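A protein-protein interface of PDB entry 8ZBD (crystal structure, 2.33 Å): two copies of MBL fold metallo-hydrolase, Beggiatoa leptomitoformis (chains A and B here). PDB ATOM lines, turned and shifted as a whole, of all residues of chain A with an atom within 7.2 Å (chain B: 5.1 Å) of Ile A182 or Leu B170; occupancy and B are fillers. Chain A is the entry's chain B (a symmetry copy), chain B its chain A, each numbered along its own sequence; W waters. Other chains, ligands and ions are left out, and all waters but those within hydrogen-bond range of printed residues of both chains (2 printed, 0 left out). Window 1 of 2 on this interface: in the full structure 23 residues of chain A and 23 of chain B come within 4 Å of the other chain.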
ATOM      1  N   PHE A   3     -10.101  13.053 -16.151  1.00  0.00           N
ATOM      2  CA  PHE A   3      -9.514  13.554 -17.386  1.00  0.00           C
ATOM      3  C   PHE A   3     -10.452  13.346 -18.575  1.00  0.00           C
ATOM      4  O   PHE A   3     -10.926  12.238 -18.811  1.00  0.00           O
ATOM      5  CB  PHE A   3      -8.174  12.870 -17.655  1.00  0.00           C
ATOM      6  CG  PHE A   3      -7.569  13.266 -18.968  1.00  0.00           C
ATOM      7  CD1 PHE A   3      -7.153  14.575 -19.181  1.00  0.00           C
ATOM      8  CD2 PHE A   3      -7.447  12.345 -20.002  1.00  0.00           C
ATOM      9  CE1 PHE A   3      -6.613  14.947 -20.400  1.00  0.00           C
ATOM     10  CE2 PHE A   3      -6.906  12.700 -21.216  1.00  0.00           C
ATOM     11  CZ  PHE A   3      -6.490  14.005 -21.426  1.00  0.00           C
ATOM     12  N   GLN A   5     -10.785  14.541 -22.860  1.00  0.00           N
ATOM     13  CA  GLN A   5     -10.281  15.249 -24.032  1.00  0.00           C
ATOM     14  C   GLN A   5     -11.451  15.647 -24.922  1.00  0.00           C
ATOM     15  O   GLN A   5     -12.142  14.775 -25.450  1.00  0.00           O
ATOM     16  CB  GLN A   5      -9.300  14.379 -24.808  1.00  0.00           C
ATOM     17  CG  GLN A   5      -8.793  15.029 -26.072  1.00  0.00           C
ATOM     18  CD  GLN A   5      -7.595  14.304 -26.639  1.00  0.00           C
ATOM     19  OE1 GLN A   5      -7.340  13.171 -26.282  1.00  0.00           O
ATOM     20  NE2 GLN A   5      -6.868  14.950 -27.531  1.00  0.00           N
ATOM     21  N   TYR A  14      -8.445  21.079 -29.244  1.00  0.00           N
ATOM     22  CA  TYR A  14      -8.662  20.176 -28.126  1.00  0.00           C
ATOM     23  C   TYR A  14      -8.691  20.988 -26.845  1.00  0.00           C
ATOM     24  O   TYR A  14      -7.762  21.742 -26.569  1.00  0.00           O
ATOM     25  CB  TYR A  14      -7.580  19.088 -28.044  1.00  0.00           C
ATOM     26  CG  TYR A  14      -7.765  17.941 -29.005  1.00  0.00           C
ATOM     27  CD1 TYR A  14      -8.906  17.152 -28.971  1.00  0.00           C
ATOM     28  CD2 TYR A  14      -6.792  17.642 -29.948  1.00  0.00           C
ATOM     29  CE1 TYR A  14      -9.072  16.086 -29.864  1.00  0.00           C
ATOM     30  CE2 TYR A  14      -6.952  16.595 -30.838  1.00  0.00           C
ATOM     31  CZ  TYR A  14      -8.088  15.820 -30.789  1.00  0.00           C
ATOM     32  OH  TYR A  14      -8.221  14.785 -31.681  1.00  0.00           O
ATOM     33  N   TYR A  16      -8.865  20.396 -22.727  1.00  0.00           N
ATOM     34  CA  TYR A  16      -8.558  19.332 -21.778  1.00  0.00           C
ATOM     35  C   TYR A  16      -9.164  19.671 -20.427  1.00  0.00           C
ATOM     36  O   TYR A  16      -8.849  20.713 -19.839  1.00  0.00           O
ATOM     37  CB  TYR A  16      -7.057  19.103 -21.671  1.00  0.00           C
ATOM     38  CG  TYR A  16      -6.520  18.626 -22.981  1.00  0.00           C
ATOM     39  CD1 TYR A  16      -6.602  17.276 -23.331  1.00  0.00           C
ATOM     40  CD2 TYR A  16      -5.955  19.526 -23.900  1.00  0.00           C
ATOM     41  CE1 TYR A  16      -6.116  16.818 -24.557  1.00  0.00           C
ATOM     42  CE2 TYR A  16      -5.463  19.077 -25.129  1.00  0.00           C
ATOM     43  CZ  TYR A  16      -5.545  17.724 -25.461  1.00  0.00           C
ATOM     44  OH  TYR A  16      -5.064  17.265 -26.683  1.00  0.00           O
ATOM     45  N   HIS A 127       2.267   8.050 -15.827  1.00  0.00           N
ATOM     46  CA  HIS A 127       2.563   8.795 -17.044  1.00  0.00           C
ATOM     47  C   HIS A 127       2.790  10.266 -16.721  1.00  0.00           C
ATOM     48  O   HIS A 127       2.152  10.820 -15.817  1.00  0.00           O
ATOM     49  CB  HIS A 127       1.416   8.756 -18.055  1.00  0.00           C
ATOM     50  CG  HIS A 127       1.113   7.398 -18.594  1.00  0.00           C
ATOM     51  ND1 HIS A 127       0.266   6.513 -17.953  1.00  0.00           N
ATOM     52  CD2 HIS A 127       1.508   6.785 -19.735  1.00  0.00           C
ATOM     53  CE1 HIS A 127       0.171   5.405 -18.670  1.00  0.00           C
ATOM     54  NE2 HIS A 127       0.911   5.545 -19.756  1.00  0.00           N
ATOM     55  N   ILE A 138       0.836  16.521 -33.552  1.00  0.00           N
ATOM     56  CA  ILE A 138       1.032  15.128 -33.953  1.00  0.00           C
ATOM     57  C   ILE A 138       1.458  15.102 -35.416  1.00  0.00           C
ATOM     58  O   ILE A 138       0.698  15.499 -36.306  1.00  0.00           O
ATOM     59  CB  ILE A 138      -0.216  14.275 -33.714  1.00  0.00           C
ATOM     60  CG1 ILE A 138      -0.646  14.417 -32.254  1.00  0.00           C
ATOM     61  CG2 ILE A 138       0.089  12.817 -34.040  1.00  0.00           C
ATOM     62  CD1 ILE A 138      -1.892  13.685 -31.899  1.00  0.00           C
ATOM     63  N   THR A 169       6.264   9.811 -22.250  1.00  0.00           N
ATOM     64  CA  THR A 169       5.446  11.000 -22.072  1.00  0.00           C
ATOM     65  C   THR A 169       4.326  11.046 -23.103  1.00  0.00           C
ATOM     66  O   THR A 169       4.573  10.936 -24.303  1.00  0.00           O
ATOM     67  CB  THR A 169       6.314  12.258 -22.190  1.00  0.00           C
ATOM     68  OG1 THR A 169       7.323  12.252 -21.164  1.00  0.00           O
ATOM     69  CG2 THR A 169       5.454  13.502 -22.062  1.00  0.00           C
ATOM     70  N   LEU A 170       3.092  11.211 -22.626  1.00  0.00           N
ATOM     71  CA  LEU A 170       1.946  11.371 -23.509  1.00  0.00           C
ATOM     72  C   LEU A 170       1.889  12.784 -24.098  1.00  0.00           C
ATOM     73  O   LEU A 170       2.024  13.774 -23.373  1.00  0.00           O
ATOM     74  CB  LEU A 170       0.656  11.072 -22.742  1.00  0.00           C
ATOM     75  CG  LEU A 170       0.619   9.761 -21.962  1.00  0.00           C
ATOM     76  CD1 LEU A 170      -0.741   9.601 -21.266  1.00  0.00           C
ATOM     77  CD2 LEU A 170       0.900   8.613 -22.911  1.00  0.00           C
ATOM     78  N   VAL A 171       1.663  12.876 -25.407  1.00  0.00           N
ATOM     79  CA  VAL A 171       1.550  14.154 -26.107  1.00  0.00           C
ATOM     80  C   VAL A 171       0.084  14.392 -26.438  1.00  0.00           C
ATOM     81  O   VAL A 171      -0.471  13.733 -27.326  1.00  0.00           O
ATOM     82  CB  VAL A 171       2.394  14.205 -27.390  1.00  0.00           C
ATOM     83  CG1 VAL A 171       2.083  15.500 -28.146  1.00  0.00           C
ATOM     84  CG2 VAL A 171       3.892  14.091 -27.088  1.00  0.00           C
ATOM     85  N   TYR A 172      -0.526  15.377 -25.768  1.00  0.00           N
ATOM     86  CA  TYR A 172      -1.895  15.821 -26.027  1.00  0.00           C
ATOM     87  C   TYR A 172      -1.864  17.178 -26.732  1.00  0.00           C
ATOM     88  O   TYR A 172      -1.644  18.208 -26.086  1.00  0.00           O
ATOM     89  CB  TYR A 172      -2.668  15.917 -24.711  1.00  0.00           C
ATOM     90  CG  TYR A 172      -3.061  14.579 -24.118  1.00  0.00           C
ATOM     91  CD1 TYR A 172      -4.069  13.806 -24.703  1.00  0.00           C
ATOM     92  CD2 TYR A 172      -2.429  14.083 -22.982  1.00  0.00           C
ATOM     93  CE1 TYR A 172      -4.439  12.585 -24.164  1.00  0.00           C
ATOM     94  CE2 TYR A 172      -2.793  12.859 -22.433  1.00  0.00           C
ATOM     95  CZ  TYR A 172      -3.796  12.113 -23.029  1.00  0.00           C
ATOM     96  OH  TYR A 172      -4.166  10.895 -22.506  1.00  0.00           O
ATOM     97  N   PRO A 173      -2.087  17.240 -28.038  1.00  0.00           N
ATOM     98  CA  PRO A 173      -1.845  18.483 -28.778  1.00  0.00           C
ATOM     99  C   PRO A 173      -2.977  19.495 -28.626  1.00  0.00           C
ATOM    100  O   PRO A 173      -4.103  19.176 -28.222  1.00  0.00           O
ATOM    101  CB  PRO A 173      -1.755  17.991 -30.226  1.00  0.00           C
ATOM    102  CG  PRO A 173      -2.783  16.888 -30.254  1.00  0.00           C
ATOM    103  CD  PRO A 173      -2.593  16.171 -28.922  1.00  0.00           C
ATOM    104  N   ASP A 176      -5.693  19.090 -33.931  1.00  0.00           N
ATOM    105  CA  ASP A 176      -5.413  18.032 -34.892  1.00  0.00           C
ATOM    106  C   ASP A 176      -6.463  18.138 -35.984  1.00  0.00           C
ATOM    107  O   ASP A 176      -7.648  18.366 -35.702  1.00  0.00           O
ATOM    108  CB  ASP A 176      -5.425  16.620 -34.273  1.00  0.00           C
ATOM    109  CG  ASP A 176      -4.763  15.556 -35.191  1.00  0.00           C
ATOM    110  OD1 ASP A 176      -3.511  15.461 -35.201  1.00  0.00           O
ATOM    111  OD2 ASP A 176      -5.485  14.811 -35.904  1.00  0.00           O
ATOM    112  N   GLY A 179      -8.069  13.615 -37.078  1.00  0.00           N
ATOM    113  CA  GLY A 179      -8.670  12.622 -36.208  1.00  0.00           C
ATOM    114  C   GLY A 179      -7.727  11.930 -35.252  1.00  0.00           C
ATOM    115  O   GLY A 179      -8.100  10.900 -34.675  1.00  0.00           O
ATOM    116  N   ARG A 180      -6.515  12.440 -35.073  1.00  0.00           N
ATOM    117  CA  ARG A 180      -5.593  11.868 -34.107  1.00  0.00           C
ATOM    118  C   ARG A 180      -5.764  12.598 -32.780  1.00  0.00           C
ATOM    119  O   ARG A 180      -5.982  13.818 -32.745  1.00  0.00           O
ATOM    120  CB  ARG A 180      -4.156  11.959 -34.624  1.00  0.00           C
ATOM    121  CG  ARG A 180      -3.998  11.335 -36.031  1.00  0.00           C
ATOM    122  CD  ARG A 180      -2.544  11.098 -36.444  1.00  0.00           C
ATOM    123  NE  ARG A 180      -2.259  11.530 -37.815  1.00  0.00           N
ATOM    124  CZ  ARG A 180      -1.997  12.783 -38.216  1.00  0.00           C
ATOM    125  NH1 ARG A 180      -2.033  13.827 -37.380  1.00  0.00           N
ATOM    126  NH2 ARG A 180      -1.687  13.001 -39.493  1.00  0.00           N
ATOM    127  N   PHE A 181      -5.730  11.840 -31.686  1.00  0.00           N
ATOM    128  CA  PHE A 181      -5.946  12.409 -30.362  1.00  0.00           C
ATOM    129  C   PHE A 181      -4.684  12.480 -29.509  1.00  0.00           C
ATOM    130  O   PHE A 181      -4.570  13.366 -28.651  1.00  0.00           O
ATOM    131  CB  PHE A 181      -7.000  11.596 -29.596  1.00  0.00           C
ATOM    132  CG  PHE A 181      -8.406  11.749 -30.116  1.00  0.00           C
ATOM    133  CD1 PHE A 181      -8.754  11.301 -31.392  1.00  0.00           C
ATOM    134  CD2 PHE A 181      -9.400  12.309 -29.311  1.00  0.00           C
ATOM    135  CE1 PHE A 181     -10.061  11.420 -31.883  1.00  0.00           C
ATOM    136  CE2 PHE A 181     -10.718  12.418 -29.792  1.00  0.00           C
ATOM    137  CZ  PHE A 181     -11.037  11.969 -31.085  1.00  0.00           C
ATOM    138  N   ILE A 182      -3.732  11.575 -29.710  1.00  0.00           N
ATOM    139  CA  ILE A 182      -2.643  11.422 -28.761  1.00  0.00           C
ATOM    140  C   ILE A 182      -1.416  10.936 -29.501  1.00  0.00           C
ATOM    141  O   ILE A 182      -1.510  10.226 -30.507  1.00  0.00           O
ATOM    142  CB  ILE A 182      -3.022  10.448 -27.616  1.00  0.00           C
ATOM    143  CG1 ILE A 182      -1.976  10.499 -26.499  1.00  0.00           C
ATOM    144  CG2 ILE A 182      -3.247   9.007 -28.147  1.00  0.00           C
ATOM    145  CD1 ILE A 182      -2.350   9.683 -25.273  1.00  0.00           C
ATOM    146  N   SER A 183      -0.256  11.323 -28.990  1.00  0.00           N
ATOM    147  CA  SER A 183       1.014  10.738 -29.389  1.00  0.00           C
ATOM    148  C   SER A 183       1.824  10.537 -28.118  1.00  0.00           C
ATOM    149  O   SER A 183       1.301  10.657 -27.008  1.00  0.00           O
ATOM    150  CB  SER A 183       1.743  11.623 -30.417  1.00  0.00           C
ATOM    151  OG  SER A 183       2.769  10.906 -31.096  1.00  0.00           O
ATOM    152  N   SER A 184       3.103  10.214 -28.295  1.00  0.00           N
ATOM    153  CA  SER A 184       4.085  10.146 -27.222  1.00  0.00           C
ATOM    154  C   SER A 184       5.347  10.845 -27.701  1.00  0.00           C
ATOM    155  O   SER A 184       5.534  11.073 -28.900  1.00  0.00           O
ATOM    156  CB  SER A 184       4.412   8.701 -26.814  1.00  0.00           C
ATOM    157  OG  SER A 184       5.171   8.024 -27.816  1.00  0.00           O
ATOM    158  N   GLN A 187       7.256   8.637 -30.041  1.00  0.00           N
ATOM    159  CA  GLN A 187       6.689   8.574 -31.383  1.00  0.00           C
ATOM    160  C   GLN A 187       7.040   9.813 -32.202  1.00  0.00           C
ATOM    161  O   GLN A 187       7.406   9.701 -33.380  1.00  0.00           O
ATOM    162  CB  GLN A 187       5.180   8.394 -31.294  1.00  0.00           C
ATOM    163  CG  GLN A 187       4.455   8.475 -32.603  1.00  0.00           C
ATOM    164  CD  GLN A 187       3.015   8.011 -32.460  1.00  0.00           C
ATOM    165  OE1 GLN A 187       2.718   7.143 -31.636  1.00  0.00           O
ATOM    166  NE2 GLN A 187       2.109   8.587 -33.258  1.00  0.00           N
ATOM    167  N   GLU A 188       6.928  11.007 -31.607  1.00  0.00           N
ATOM    168  CA  GLU A 188       7.270  12.208 -32.360  1.00  0.00           C
ATOM    169  C   GLU A 188       8.751  12.229 -32.751  1.00  0.00           C
ATOM    170  O   GLU A 188       9.087  12.576 -33.888  1.00  0.00           O
ATOM    171  CB  GLU A 188       6.870  13.459 -31.579  1.00  0.00           C
ATOM    172  CG  GLU A 188       5.347  13.677 -31.494  1.00  0.00           C
ATOM    173  CD  GLU A 188       4.597  13.414 -32.818  1.00  0.00           C
ATOM    174  OE1 GLU A 188       4.870  14.116 -33.820  1.00  0.00           O
ATOM    175  OE2 GLU A 188       3.714  12.510 -32.850  1.00  0.00           O
ATOM    176  N   HIS B 127      -5.596   6.944 -16.267  1.00  0.00           N
ATOM    177  CA  HIS B 127      -5.807   6.280 -17.537  1.00  0.00           C
ATOM    178  C   HIS B 127      -6.109   4.804 -17.332  1.00  0.00           C
ATOM    179  O   HIS B 127      -5.616   4.177 -16.386  1.00  0.00           O
ATOM    180  CB  HIS B 127      -4.586   6.397 -18.433  1.00  0.00           C
ATOM    181  CG  HIS B 127      -4.207   7.804 -18.743  1.00  0.00           C
ATOM    182  ND1 HIS B 127      -4.692   8.476 -19.842  1.00  0.00           N
ATOM    183  CD2 HIS B 127      -3.383   8.665 -18.108  1.00  0.00           C
ATOM    184  CE1 HIS B 127      -4.192   9.697 -19.866  1.00  0.00           C
ATOM    185  NE2 HIS B 127      -3.391   9.836 -18.827  1.00  0.00           N
ATOM    186  N   LEU B 128      -6.942   4.269 -18.224  1.00  0.00           N
ATOM    187  CA  LEU B 128      -6.935   2.852 -18.543  1.00  0.00           C
ATOM    188  C   LEU B 128      -5.908   2.651 -19.647  1.00  0.00           C
ATOM    189  O   LEU B 128      -5.972   3.335 -20.678  1.00  0.00           O
ATOM    190  CB  LEU B 128      -8.306   2.390 -19.031  1.00  0.00           C
ATOM    191  CG  LEU B 128      -9.149   1.482 -18.164  1.00  0.00           C
ATOM    192  CD1 LEU B 128      -9.028   1.907 -16.710  1.00  0.00           C
ATOM    193  CD2 LEU B 128     -10.583   1.556 -18.646  1.00  0.00           C
ATOM    194  N   MET B 129      -4.954   1.747 -19.417  1.00  0.00           N
ATOM    195  CA  MET B 129      -3.949   1.378 -20.403  1.00  0.00           C
ATOM    196  C   MET B 129      -4.367   0.039 -21.016  1.00  0.00           C
ATOM    197  O   MET B 129      -4.420  -0.971 -20.306  1.00  0.00           O
ATOM    198  CB  MET B 129      -2.572   1.213 -19.762  1.00  0.00           C
ATOM    199  CG  MET B 129      -2.152   2.242 -18.765  1.00  0.00           C
ATOM    200  SD  MET B 129      -0.465   1.936 -18.116  1.00  0.00           S
ATOM    201  CE  MET B 129       0.537   2.044 -19.586  1.00  0.00           C
ATOM    202  N   LEU B 130      -4.623   0.012 -22.326  1.00  0.00           N
ATOM    203  CA  LEU B 130      -4.995  -1.219 -23.001  1.00  0.00           C
ATOM    204  C   LEU B 130      -3.805  -1.743 -23.798  1.00  0.00           C
ATOM    205  O   LEU B 130      -3.381  -1.130 -24.782  1.00  0.00           O
ATOM    206  CB  LEU B 130      -6.205  -1.009 -23.901  1.00  0.00           C
ATOM    207  CG  LEU B 130      -6.504  -2.151 -24.865  1.00  0.00           C
ATOM    208  CD1 LEU B 130      -7.088  -3.331 -24.107  1.00  0.00           C
ATOM    209  CD2 LEU B 130      -7.462  -1.666 -25.934  1.00  0.00           C
ATOM    210  N   GLU B 168     -10.768   7.949 -23.555  1.00  0.00           N
ATOM    211  CA  GLU B 168      -9.390   8.293 -23.236  1.00  0.00           C
ATOM    212  C   GLU B 168      -8.506   7.067 -22.985  1.00  0.00           C
ATOM    213  O   GLU B 168      -7.325   7.231 -22.656  1.00  0.00           O
ATOM    214  CB  GLU B 168      -9.367   9.221 -22.019  1.00  0.00           C
ATOM    215  CG  GLU B 168      -9.885  10.632 -22.294  1.00  0.00           C
ATOM    216  CD  GLU B 168     -11.406  10.708 -22.422  1.00  0.00           C
ATOM    217  OE1 GLU B 168     -12.105   9.798 -21.907  1.00  0.00           O
ATOM    218  OE2 GLU B 168     -11.901  11.658 -23.072  1.00  0.00           O
ATOM    219  N   THR B 169      -9.040   5.856 -23.134  1.00  0.00           N
ATOM    220  CA  THR B 169      -8.247   4.645 -22.941  1.00  0.00           C
ATOM    221  C   THR B 169      -7.051   4.624 -23.890  1.00  0.00           C
ATOM    222  O   THR B 169      -7.204   4.769 -25.103  1.00  0.00           O
ATOM    223  CB  THR B 169      -9.131   3.410 -23.173  1.00  0.00           C
ATOM    224  OG1 THR B 169     -10.234   3.440 -22.269  1.00  0.00           O
ATOM    225  CG2 THR B 169      -8.359   2.132 -22.977  1.00  0.00           C
ATOM    226  N   LEU B 170      -5.858   4.423 -23.331  1.00  0.00           N
ATOM    227  CA  LEU B 170      -4.642   4.345 -24.131  1.00  0.00           C
ATOM    228  C   LEU B 170      -4.543   2.986 -24.817  1.00  0.00           C
ATOM    229  O   LEU B 170      -4.855   1.945 -24.226  1.00  0.00           O
ATOM    230  CB  LEU B 170      -3.413   4.585 -23.251  1.00  0.00           C
ATOM    231  CG  LEU B 170      -3.467   5.811 -22.343  1.00  0.00           C
ATOM    232  CD1 LEU B 170      -2.259   5.865 -21.415  1.00  0.00           C
ATOM    233  CD2 LEU B 170      -3.570   7.086 -23.170  1.00  0.00           C
ATOM    234  N   VAL B 171      -4.115   2.992 -26.072  1.00  0.00           N
ATOM    235  CA  VAL B 171      -4.004   1.780 -26.872  1.00  0.00           C
ATOM    236  C   VAL B 171      -2.520   1.525 -27.074  1.00  0.00           C
ATOM    237  O   VAL B 171      -1.859   2.244 -27.835  1.00  0.00           O
ATOM    238  CB  VAL B 171      -4.725   1.908 -28.223  1.00  0.00           C
ATOM    239  CG1 VAL B 171      -4.399   0.742 -29.108  1.00  0.00           C
ATOM    240  CG2 VAL B 171      -6.229   2.037 -28.050  1.00  0.00           C
ATOM    241  N   TYR B 172      -1.990   0.507 -26.398  1.00  0.00           N
ATOM    242  CA  TYR B 172      -0.590   0.117 -26.551  1.00  0.00           C
ATOM    243  C   TYR B 172      -0.530  -1.170 -27.369  1.00  0.00           C
ATOM    244  O   TYR B 172      -0.837  -2.254 -26.846  1.00  0.00           O
ATOM    245  CB  TYR B 172       0.062  -0.072 -25.177  1.00  0.00           C
ATOM    246  CG  TYR B 172       0.419   1.249 -24.486  1.00  0.00           C
ATOM    247  CD1 TYR B 172       1.509   2.012 -24.904  1.00  0.00           C
ATOM    248  CD2 TYR B 172      -0.342   1.731 -23.435  1.00  0.00           C
ATOM    249  CE1 TYR B 172       1.831   3.217 -24.279  1.00  0.00           C
ATOM    250  CE2 TYR B 172      -0.029   2.936 -22.799  1.00  0.00           C
ATOM    251  CZ  TYR B 172       1.060   3.671 -23.225  1.00  0.00           C
ATOM    252  OH  TYR B 172       1.357   4.861 -22.606  1.00  0.00           O
ATOM    253  N   ILE B 182       1.522   4.662 -29.781  1.00  0.00           N
ATOM    254  CA  ILE B 182       0.389   4.769 -28.884  1.00  0.00           C
ATOM    255  C   ILE B 182      -0.779   5.332 -29.665  1.00  0.00           C
ATOM    256  O   ILE B 182      -0.599   6.072 -30.641  1.00  0.00           O
ATOM    257  CB  ILE B 182       0.743   5.638 -27.648  1.00  0.00           C
ATOM    258  CG1 ILE B 182      -0.393   5.611 -26.627  1.00  0.00           C
ATOM    259  CG2 ILE B 182       1.016   7.080 -28.039  1.00  0.00           C
ATOM    260  CD1 ILE B 182       0.040   6.068 -25.267  1.00  0.00           C
ATOM    261  N   SER B 183      -1.983   4.971 -29.234  1.00  0.00           N
ATOM    262  CA  SER B 183      -3.204   5.598 -29.718  1.00  0.00           C
ATOM    263  C   SER B 183      -4.211   5.633 -28.576  1.00  0.00           C
ATOM    264  O   SER B 183      -3.876   5.380 -27.416  1.00  0.00           O
ATOM    265  CB  SER B 183      -3.758   4.854 -30.936  1.00  0.00           C
ATOM    266  OG  SER B 183      -4.880   5.538 -31.452  1.00  0.00           O
ATOM    267  N   SER B 184      -5.456   5.951 -28.906  1.00  0.00           N
ATOM    268  CA  SER B 184      -6.530   5.924 -27.927  1.00  0.00           C
ATOM    269  C   SER B 184      -7.763   5.292 -28.563  1.00  0.00           C
ATOM    270  O   SER B 184      -7.899   5.251 -29.789  1.00  0.00           O
ATOM    271  CB  SER B 184      -6.869   7.329 -27.407  1.00  0.00           C
ATOM    272  OG  SER B 184      -7.604   8.035 -28.387  1.00  0.00           O
ATOM    273  N   GLN B 187      -9.397   7.723 -30.748  1.00  0.00           N
ATOM    274  CA  GLN B 187      -8.725   7.887 -32.033  1.00  0.00           C
ATOM    275  C   GLN B 187      -9.074   6.751 -32.994  1.00  0.00           C
ATOM    276  O   GLN B 187      -9.403   6.984 -34.165  1.00  0.00           O
ATOM    277  CB  GLN B 187      -7.216   7.962 -31.825  1.00  0.00           C
ATOM    278  CG  GLN B 187      -6.413   7.914 -33.122  1.00  0.00           C
ATOM    279  CD  GLN B 187      -5.017   8.463 -32.918  1.00  0.00           C
ATOM    280  OE1 GLN B 187      -4.795   9.294 -32.026  1.00  0.00           O
ATOM    281  NE2 GLN B 187      -4.068   8.010 -33.735  1.00  0.00           N
HETATM  282  O   HOH W   1      -1.063   8.365 -32.375  1.00  0.00           O
HETATM  283  O   HOH W   2      -6.227   9.859 -23.754  1.00  0.00           O
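The side-chain amide nitrogen (NE2) of Gln A187 sits close to the side-chain hydroxyl (OG) of Ser A183 (3.2 Å). N of Gln B187 is in hydrogen-bond range of OG of Ser B184, 3.0 Å away. The side-chain amide nitrogen (NE2) of Gln A5 lies within hydrogen-bond range of the backbone carbonyl oxygen (O) of Phe A181. The backbone NH (N) of Val A171 sits at hydrogen-bond distance from the backbone carbonyl oxygen (O) of Ser A183. The backbone NH (N) of Leu B170 sits at hydrogen-bond distance from the backbone carbonyl oxygen (O) of Leu B128 (2.9 Å). The backbone NH (N) of Leu B130 lies within hydrogen-bond range of the backbone carbonyl oxygen (O) of Leu B170 (2.7 Å).
Of the printed residues of chain B, Phe A3 touches Glu B168. Of the printed residues of chain B, Gln A5 touches Glu B168. Thr A169 touches none of the printed residues of chain B. Of chain B, only Leu B170 (3.6 Å), Ser B183 (3.5 Å), Ser B184 (3.8 Å) and Gln B187 (3.4 Å) come within 4 Å of Ile A182. Leu B170 touches three residues of chain A. The nearest residue of chain B that does not touch Ile A182 is Ile B182 (4.3 Å).
Printed residues of chain B that touch a printed residue of chain A: His B127, Met B129, Glu B168, Leu B170, Tyr B172, Ile B182, Ser B183, Ser B184 and Gln B187. Of the 20 printed residues of chain A, 12 touch a printed residue of chain B. Hydrophobic or aromatic side chains of chain A that line the printed part of chain B: Phe A3, His A127, Leu A170, Tyr A172, Phe A181 and Ile A182. Among the printed residues, 21 pairs touch across the chains. Among the printed residues, no Asp or Glu carboxylate lies within 4 Å of a Lys or Arg side-chain nitrogen of the other chain.
Water W2 lies within hydrogen-bond range of OH of Tyr A172 (2.6 Å) and O of Glu B168 (3.1 Å). Water W1 lies within hydrogen-bond range of the backbone carbonyl oxygen of Ile A182 (2.7 Å), the backbone carbonyl oxygen of Ile B182 (2.9 Å), the side-chain amide nitrogen of Gln A187 (3.3 Å) and the side-chain amide nitrogen of Gln B187 (3.3 Å).
Among the printed residues, merely in contact across the chains: Phe A3 with Glu B168 (3.8 Å), His A127 with Met B129 (3.5 Å), His A127 with Leu B170 (3.6 Å), Leu A170 with His B127 (3.6 Å), Leu A170 with Tyr B172 (3.8 Å), Leu A170 with Ile B182 (3.6 Å), Tyr A172 with His B127 (2.9 Å), Tyr A172 with Leu B170 (3.9 Å), Gly A179 with Gln B187 (3.8 Å), Arg A180 with Gln B187 (3.4 Å), Phe A181 with Ser B184 (3.8 Å), Ile A182 with Leu B170 (3.6 Å), Ile A182 with Ser B183 (3.5 Å), Ile A182 with Ser B184 (3.8 Å), Ser A183 with Ile B182 (3.6 Å) and Ser A184 with Ile B182 (3.8 Å).
His A127 touches Leu B170, and with the chains exchanged Leu A170 touches His B127. Ile A182 touches Ser B183, and with the chains exchanged Ser A183 touches Ile B182. Ile A182 touches Ser B184, and with the chains exchanged Ser A184 touches Ile B182. Ile A182 touches Gln B187, and with the chains exchanged Gln A187 touches Ile B182. Positions printed for both chains: 127, 169, 170, 171, 172, 182, 183, 184 and 187. Of the 21 pairs that touch across the chains among the printed residues, 14 have their exchanged pair printed and touching as well.
OH of Tyr B172 is in hydrogen-bond range of NE2 of His A127 (3.0 Å). N of Ile B182 lies within hydrogen-bond range of OE1 of Gln A187, 3.3 Å away. OE1 of Gln B187 lies within hydrogen-bond range of N of Phe A181 (2.7 Å). The side-chain carboxylate (OE2) of Glu B168 lies within hydrogen-bond range of the backbone NH (N) of Gln A5 (3.1 Å). The side-chain amide oxygen (OE1) of Gln B187 lies within hydrogen-bond range of the backbone NH (N) of Ile A182, 3.4 Å away.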
